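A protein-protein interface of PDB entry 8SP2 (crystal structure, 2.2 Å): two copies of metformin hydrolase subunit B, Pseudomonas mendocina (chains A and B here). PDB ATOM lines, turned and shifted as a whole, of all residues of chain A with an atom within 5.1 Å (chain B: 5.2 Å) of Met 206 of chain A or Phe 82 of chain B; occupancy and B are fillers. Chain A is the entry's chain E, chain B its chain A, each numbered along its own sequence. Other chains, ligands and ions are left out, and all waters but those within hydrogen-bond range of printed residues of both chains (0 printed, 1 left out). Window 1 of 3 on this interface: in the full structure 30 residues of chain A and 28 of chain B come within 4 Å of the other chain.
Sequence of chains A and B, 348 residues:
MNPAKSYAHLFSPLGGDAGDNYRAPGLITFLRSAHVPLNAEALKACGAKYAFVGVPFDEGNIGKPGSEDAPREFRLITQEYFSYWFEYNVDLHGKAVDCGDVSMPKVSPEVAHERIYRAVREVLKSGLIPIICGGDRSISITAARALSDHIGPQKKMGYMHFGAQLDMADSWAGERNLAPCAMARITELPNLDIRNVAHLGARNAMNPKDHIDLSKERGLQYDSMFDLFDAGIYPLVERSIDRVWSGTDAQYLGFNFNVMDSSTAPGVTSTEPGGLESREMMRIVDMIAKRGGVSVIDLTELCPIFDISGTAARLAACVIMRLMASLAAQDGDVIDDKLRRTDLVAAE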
ATOM      1  N   GLN A 165     -17.339 -22.204 -28.070  1.00  0.00           N
ATOM      2  CA  GLN A 165     -17.870 -21.602 -29.287  1.00  0.00           C
ATOM      3  C   GLN A 165     -17.173 -22.216 -30.504  1.00  0.00           C
ATOM      4  O   GLN A 165     -15.936 -22.308 -30.538  1.00  0.00           O
ATOM      5  CB  GLN A 165     -17.617 -20.092 -29.291  1.00  0.00           C
ATOM      6  CG  GLN A 165     -18.172 -19.346 -28.086  1.00  0.00           C
ATOM      7  CD  GLN A 165     -17.433 -18.049 -27.857  1.00  0.00           C
ATOM      8  OE1 GLN A 165     -16.484 -17.991 -27.076  1.00  0.00           O
ATOM      9  NE2 GLN A 165     -17.833 -17.005 -28.568  1.00  0.00           N
ATOM     10  N   TRP A 172     -18.979 -12.194 -40.119  1.00  0.00           N
ATOM     11  CA  TRP A 172     -19.550 -11.614 -38.917  1.00  0.00           C
ATOM     12  C   TRP A 172     -19.548 -10.092 -39.054  1.00  0.00           C
ATOM     13  O   TRP A 172     -18.481  -9.486 -39.149  1.00  0.00           O
ATOM     14  CB  TRP A 172     -18.778 -12.070 -37.660  1.00  0.00           C
ATOM     15  CG  TRP A 172     -19.429 -11.640 -36.379  1.00  0.00           C
ATOM     16  CD1 TRP A 172     -19.434 -10.390 -35.833  1.00  0.00           C
ATOM     17  CD2 TRP A 172     -20.245 -12.452 -35.517  1.00  0.00           C
ATOM     18  NE1 TRP A 172     -20.171 -10.375 -34.680  1.00  0.00           N
ATOM     19  CE2 TRP A 172     -20.695 -11.623 -34.467  1.00  0.00           C
ATOM     20  CE3 TRP A 172     -20.633 -13.796 -35.530  1.00  0.00           C
ATOM     21  CZ2 TRP A 172     -21.515 -12.099 -33.440  1.00  0.00           C
ATOM     22  CZ3 TRP A 172     -21.438 -14.266 -34.517  1.00  0.00           C
ATOM     23  CH2 TRP A 172     -21.866 -13.429 -33.484  1.00  0.00           C
ATOM     24  N   ARG A 203     -20.939 -25.600 -26.601  1.00  0.00           N
ATOM     25  CA  ARG A 203     -22.152 -25.714 -25.802  1.00  0.00           C
ATOM     26  C   ARG A 203     -22.810 -24.343 -25.681  1.00  0.00           C
ATOM     27  O   ARG A 203     -22.173 -23.342 -25.982  1.00  0.00           O
ATOM     28  CB  ARG A 203     -21.812 -26.249 -24.405  1.00  0.00           C
ATOM     29  CG  ARG A 203     -20.985 -25.287 -23.559  1.00  0.00           C
ATOM     30  CD  ARG A 203     -20.489 -25.920 -22.262  1.00  0.00           C
ATOM     31  NE  ARG A 203     -19.745 -24.989 -21.424  1.00  0.00           N
ATOM     32  CZ  ARG A 203     -18.426 -24.851 -21.442  1.00  0.00           C
ATOM     33  NH1 ARG A 203     -17.701 -25.539 -22.309  1.00  0.00           N
ATOM     34  NH2 ARG A 203     -17.828 -24.024 -20.601  1.00  0.00           N
ATOM     35  N   ASN A 204     -24.060 -24.324 -25.192  1.00  0.00           N
ATOM     36  CA  ASN A 204     -24.768 -23.106 -24.833  1.00  0.00           C
ATOM     37  C   ASN A 204     -25.034 -22.269 -26.084  1.00  0.00           C
ATOM     38  O   ASN A 204     -24.863 -22.754 -27.202  1.00  0.00           O
ATOM     39  CB  ASN A 204     -24.038 -22.384 -23.701  1.00  0.00           C
ATOM     40  CG  ASN A 204     -24.070 -23.187 -22.421  1.00  0.00           C
ATOM     41  OD1 ASN A 204     -24.964 -24.006 -22.219  1.00  0.00           O
ATOM     42  ND2 ASN A 204     -23.125 -22.934 -21.533  1.00  0.00           N
ATOM     43  N   ALA A 205     -25.453 -21.013 -25.895  1.00  0.00           N
ATOM     44  CA  ALA A 205     -26.213 -20.310 -26.914  1.00  0.00           C
ATOM     45  C   ALA A 205     -25.358 -19.375 -27.768  1.00  0.00           C
ATOM     46  O   ALA A 205     -25.917 -18.721 -28.639  1.00  0.00           O
ATOM     47  CB  ALA A 205     -27.346 -19.557 -26.262  1.00  0.00           C
ATOM     48  N   MET A 206     -24.028 -19.336 -27.570  1.00  0.00           N
ATOM     49  CA  MET A 206     -23.166 -18.459 -28.357  1.00  0.00           C
ATOM     50  C   MET A 206     -22.693 -19.187 -29.616  1.00  0.00           C
ATOM     51  O   MET A 206     -21.511 -19.181 -29.956  1.00  0.00           O
ATOM     52  CB  MET A 206     -21.944 -17.998 -27.557  1.00  0.00           C
ATOM     53  CG  MET A 206     -22.275 -17.319 -26.241  1.00  0.00           C
ATOM     54  SD  MET A 206     -23.695 -16.176 -26.251  1.00  0.00           S
ATOM     55  CE  MET A 206     -22.905 -14.752 -25.503  1.00  0.00           C
ATOM     56  N   ASN A 207     -23.641 -19.813 -30.310  1.00  0.00           N
ATOM     57  CA  ASN A 207     -23.362 -20.653 -31.456  1.00  0.00           C
ATOM     58  C   ASN A 207     -24.565 -20.538 -32.387  1.00  0.00           C
ATOM     59  O   ASN A 207     -25.482 -21.367 -32.351  1.00  0.00           O
ATOM     60  CB  ASN A 207     -23.079 -22.106 -31.067  1.00  0.00           C
ATOM     61  CG  ASN A 207     -21.743 -22.297 -30.369  1.00  0.00           C
ATOM     62  OD1 ASN A 207     -20.701 -22.199 -31.012  1.00  0.00           O
ATOM     63  ND2 ASN A 207     -21.768 -22.608 -29.077  1.00  0.00           N
ATOM     64  N   PRO A 208     -24.600 -19.481 -33.233  1.00  0.00           N
ATOM     65  CA  PRO A 208     -25.728 -19.253 -34.131  1.00  0.00           C
ATOM     66  C   PRO A 208     -25.836 -20.363 -35.175  1.00  0.00           C
ATOM     67  O   PRO A 208     -24.862 -21.064 -35.473  1.00  0.00           O
ATOM     68  CB  PRO A 208     -25.453 -17.880 -34.765  1.00  0.00           C
ATOM     69  CG  PRO A 208     -24.313 -17.281 -33.948  1.00  0.00           C
ATOM     70  CD  PRO A 208     -23.561 -18.457 -33.367  1.00  0.00           C
ATOM     71  N   SER A 270     -15.479 -14.951 -22.310  1.00  0.00           N
ATOM     72  CA  SER A 270     -16.870 -15.389 -22.306  1.00  0.00           C
ATOM     73  C   SER A 270     -17.057 -16.709 -21.543  1.00  0.00           C
ATOM     74  O   SER A 270     -17.158 -17.775 -22.145  1.00  0.00           O
ATOM     75  CB  SER A 270     -17.376 -15.440 -23.739  1.00  0.00           C
ATOM     76  OG  SER A 270     -18.788 -15.470 -23.773  1.00  0.00           O
ATOM     77  N   GLU A 272     -18.688 -19.847 -19.511  1.00  0.00           N
ATOM     78  CA  GLU A 272     -19.830 -20.677 -19.847  1.00  0.00           C
ATOM     79  C   GLU A 272     -19.958 -21.776 -18.801  1.00  0.00           C
ATOM     80  O   GLU A 272     -18.998 -22.498 -18.528  1.00  0.00           O
ATOM     81  CB  GLU A 272     -19.654 -21.280 -21.245  1.00  0.00           C
ATOM     82  CG  GLU A 272     -19.823 -20.300 -22.389  1.00  0.00           C
ATOM     83  CD  GLU A 272     -21.232 -19.781 -22.622  1.00  0.00           C
ATOM     84  OE1 GLU A 272     -22.149 -20.125 -21.828  1.00  0.00           O
ATOM     85  OE2 GLU A 272     -21.406 -19.020 -23.598  1.00  0.00           O
ATOM     86  N   LEU B  31     -33.890 -11.364 -21.219  1.00  0.00           N
ATOM     87  CA  LEU B  31     -33.604 -11.889 -22.547  1.00  0.00           C
ATOM     88  C   LEU B  31     -33.878 -10.850 -23.642  1.00  0.00           C
ATOM     89  O   LEU B  31     -34.059 -11.212 -24.797  1.00  0.00           O
ATOM     90  CB  LEU B  31     -34.438 -13.158 -22.752  1.00  0.00           C
ATOM     91  CG  LEU B  31     -33.677 -14.471 -22.632  1.00  0.00           C
ATOM     92  CD1 LEU B  31     -34.647 -15.649 -22.544  1.00  0.00           C
ATOM     93  CD2 LEU B  31     -32.732 -14.630 -23.817  1.00  0.00           C
ATOM     94  N   ARG B  32     -33.843  -9.559 -23.288  1.00  0.00           N
ATOM     95  CA  ARG B  32     -34.223  -8.479 -24.185  1.00  0.00           C
ATOM     96  C   ARG B  32     -35.656  -8.695 -24.666  1.00  0.00           C
ATOM     97  O   ARG B  32     -36.002  -8.380 -25.797  1.00  0.00           O
ATOM     98  CB  ARG B  32     -33.246  -8.383 -25.355  1.00  0.00           C
ATOM     99  CG  ARG B  32     -31.821  -8.070 -24.935  1.00  0.00           C
ATOM    100  CD  ARG B  32     -30.840  -8.589 -25.959  1.00  0.00           C
ATOM    101  NE  ARG B  32     -31.080 -10.020 -26.056  1.00  0.00           N
ATOM    102  CZ  ARG B  32     -30.489 -10.849 -26.902  1.00  0.00           C
ATOM    103  NH1 ARG B  32     -29.404 -10.474 -27.558  1.00  0.00           N
ATOM    104  NH2 ARG B  32     -30.964 -12.078 -27.037  1.00  0.00           N
ATOM    105  N   GLU B  80     -26.963 -10.866 -22.608  1.00  0.00           N
ATOM    106  CA  GLU B  80     -25.756 -11.208 -23.336  1.00  0.00           C
ATOM    107  C   GLU B  80     -25.974 -12.393 -24.272  1.00  0.00           C
ATOM    108  O   GLU B  80     -25.166 -12.590 -25.175  1.00  0.00           O
ATOM    109  CB  GLU B  80     -24.633 -11.639 -22.393  1.00  0.00           C
ATOM    110  CG  GLU B  80     -24.306 -10.645 -21.301  1.00  0.00           C
ATOM    111  CD  GLU B  80     -23.122 -11.083 -20.451  1.00  0.00           C
ATOM    112  OE1 GLU B  80     -22.499 -12.124 -20.789  1.00  0.00           O
ATOM    113  OE2 GLU B  80     -22.806 -10.377 -19.467  1.00  0.00           O
ATOM    114  N   TYR B  81     -27.007 -13.206 -24.020  1.00  0.00           N
ATOM    115  CA  TYR B  81     -27.117 -14.502 -24.670  1.00  0.00           C
ATOM    116  C   TYR B  81     -27.911 -14.376 -25.965  1.00  0.00           C
ATOM    117  O   TYR B  81     -28.959 -13.738 -25.989  1.00  0.00           O
ATOM    118  CB  TYR B  81     -27.784 -15.527 -23.747  1.00  0.00           C
ATOM    119  CG  TYR B  81     -26.889 -16.123 -22.688  1.00  0.00           C
ATOM    120  CD1 TYR B  81     -26.623 -15.447 -21.506  1.00  0.00           C
ATOM    121  CD2 TYR B  81     -26.301 -17.367 -22.864  1.00  0.00           C
ATOM    122  CE1 TYR B  81     -25.809 -15.996 -20.525  1.00  0.00           C
ATOM    123  CE2 TYR B  81     -25.479 -17.926 -21.896  1.00  0.00           C
ATOM    124  CZ  TYR B  81     -25.231 -17.239 -20.721  1.00  0.00           C
ATOM    125  OH  TYR B  81     -24.420 -17.786 -19.757  1.00  0.00           O
ATOM    126  N   PHE B  82     -27.409 -15.021 -27.023  1.00  0.00           N
ATOM    127  CA  PHE B  82     -28.200 -15.275 -28.214  1.00  0.00           C
ATOM    128  C   PHE B  82     -29.377 -16.166 -27.835  1.00  0.00           C
ATOM    129  O   PHE B  82     -29.337 -16.859 -26.819  1.00  0.00           O
ATOM    130  CB  PHE B  82     -27.359 -15.926 -29.320  1.00  0.00           C
ATOM    131  CG  PHE B  82     -26.171 -15.117 -29.783  1.00  0.00           C
ATOM    132  CD1 PHE B  82     -24.949 -15.722 -30.042  1.00  0.00           C
ATOM    133  CD2 PHE B  82     -26.265 -13.740 -29.951  1.00  0.00           C
ATOM    134  CE1 PHE B  82     -23.857 -14.970 -30.458  1.00  0.00           C
ATOM    135  CE2 PHE B  82     -25.177 -12.993 -30.376  1.00  0.00           C
ATOM    136  CZ  PHE B  82     -23.974 -13.608 -30.621  1.00  0.00           C
ATOM    137  N   SER B  83     -30.414 -16.147 -28.672  1.00  0.00           N
ATOM    138  CA  SER B  83     -31.686 -16.754 -28.339  1.00  0.00           C
ATOM    139  C   SER B  83     -31.782 -18.152 -28.942  1.00  0.00           C
ATOM    140  O   SER B  83     -32.732 -18.888 -28.655  1.00  0.00           O
ATOM    141  CB  SER B  83     -32.821 -15.869 -28.777  1.00  0.00           C
ATOM    142  OG  SER B  83     -32.766 -15.612 -30.170  1.00  0.00           O
ATOM    143  N   TYR B  84     -30.776 -18.540 -29.742  1.00  0.00           N
ATOM    144  CA  TYR B  84     -30.821 -19.839 -30.391  1.00  0.00           C
ATOM    145  C   TYR B  84     -29.875 -20.803 -29.695  1.00  0.00           C
ATOM    146  O   TYR B  84     -28.685 -20.513 -29.560  1.00  0.00           O
ATOM    147  CB  TYR B  84     -30.458 -19.763 -31.872  1.00  0.00           C
ATOM    148  CG  TYR B  84     -30.467 -21.096 -32.579  1.00  0.00           C
ATOM    149  CD1 TYR B  84     -31.650 -21.773 -32.825  1.00  0.00           C
ATOM    150  CD2 TYR B  84     -29.285 -21.705 -32.968  1.00  0.00           C
ATOM    151  CE1 TYR B  84     -31.661 -23.003 -33.468  1.00  0.00           C
ATOM    152  CE2 TYR B  84     -29.276 -22.935 -33.602  1.00  0.00           C
ATOM    153  CZ  TYR B  84     -30.467 -23.581 -33.872  1.00  0.00           C
ATOM    154  OH  TYR B  84     -30.464 -24.799 -34.518  1.00  0.00           O
ATOM    155  N   TRP B  85     -30.418 -21.981 -29.353  1.00  0.00           N
ATOM    156  CA  TRP B  85     -29.703 -23.009 -28.616  1.00  0.00           C
ATOM    157  C   TRP B  85     -29.489 -24.229 -29.506  1.00  0.00           C
ATOM    158  O   TRP B  85     -30.390 -25.053 -29.630  1.00  0.00           O
ATOM    159  CB  TRP B  85     -30.490 -23.376 -27.358  1.00  0.00           C
ATOM    160  CG  TRP B  85     -30.478 -22.297 -26.325  1.00  0.00           C
ATOM    161  CD1 TRP B  85     -31.202 -21.138 -26.319  1.00  0.00           C
ATOM    162  CD2 TRP B  85     -29.657 -22.267 -25.145  1.00  0.00           C
ATOM    163  NE1 TRP B  85     -30.902 -20.399 -25.205  1.00  0.00           N
ATOM    164  CE2 TRP B  85     -29.956 -21.068 -24.469  1.00  0.00           C
ATOM    165  CE3 TRP B  85     -28.718 -23.144 -24.592  1.00  0.00           C
ATOM    166  CZ2 TRP B  85     -29.327 -20.722 -23.273  1.00  0.00           C
ATOM    167  CZ3 TRP B  85     -28.095 -22.796 -23.415  1.00  0.00           C
ATOM    168  CH2 TRP B  85     -28.393 -21.597 -22.769  1.00  0.00           C
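Of chain B, only Glu 80 and Phe 82 come within 4 Å of Met 206 of chain A.
Printed residues of chain B within 4 Å of Ala 205 of chain A: Phe 82 (3.2 Å), Tyr 84 (3.4 Å) and Trp 85 (3.5 Å).
Of the printed residues of chain B, Trp 172 of chain A touches Phe 82 (3.6 Å).
Ser 270 of chain A touches none of the printed residues of chain B.
Arg 203 of chain A touches none of the printed residues of chain B.
The nearest residue of chain A that does not touch Phe 82 of chain B is Pro 208 of chain A (4.2 Å).
Hydrophobic or aromatic side chains of chain B that line the printed part of chain A: Tyr 81, Phe 82, Tyr 84 and Trp 85.
Hydrophobic or aromatic side chains of chain A that line the printed part of chain B: Trp 172, Ala 205 and Met 206.
Among the printed residues, no Asp or Glu carboxylate lies within 4 Å of a Lys or Arg side-chain nitrogen of the other chain.
No position is printed for both chains.
Of the 9 pairs that touch across the chains among the printed residues, none has its exchanged pair printed and touching as well.
NH2 of Arg 203 of chain A lies within hydrogen-bond range of O of Glu 272 of chain A, at 2.8 Å.
The guanidinium group (NH2) of Arg 32 of chain B sits at hydrogen-bond distance from the backbone carbonyl oxygen (O) of Tyr 81 of chain B (2.8 Å).
The backbone carbonyl oxygen (O) of Arg 203 of chain A is in hydrogen-bond range of the side-chain amide nitrogen (ND2) of Asn 207 of chain A (3.2 Å).
ND2 of Asn 204 of chain A sits at hydrogen-bond distance from OE1 of Glu 272 of chain A, 3.0 Å away.
The backbone carbonyl oxygen (O) of Ala 205 of chain A sits close to the backbone carbonyl oxygen (O) of Tyr 84 of chain B (3.4 Å).
Among the printed residues, pairs that only touch across the chains: Trp 172 of chain A with Phe 82 of chain B (3.6 Å), Asn 204 of chain A with Trp 85 of chain B (3.6 Å), Ala 205 of chain A with Phe 82 of chain B (3.2 Å), Ala 205 of chain A with Trp 85 of chain B (3.5 Å), Met 206 of chain A with Glu 80 of chain B (3.1 Å), Met 206 of chain A with Phe 82 of chain B (3.7 Å), Asn 207 of chain A with Tyr 84 of chain B (3.9 Å) and Glu 272 of chain A with Tyr 81 of chain B (3.9 Å).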
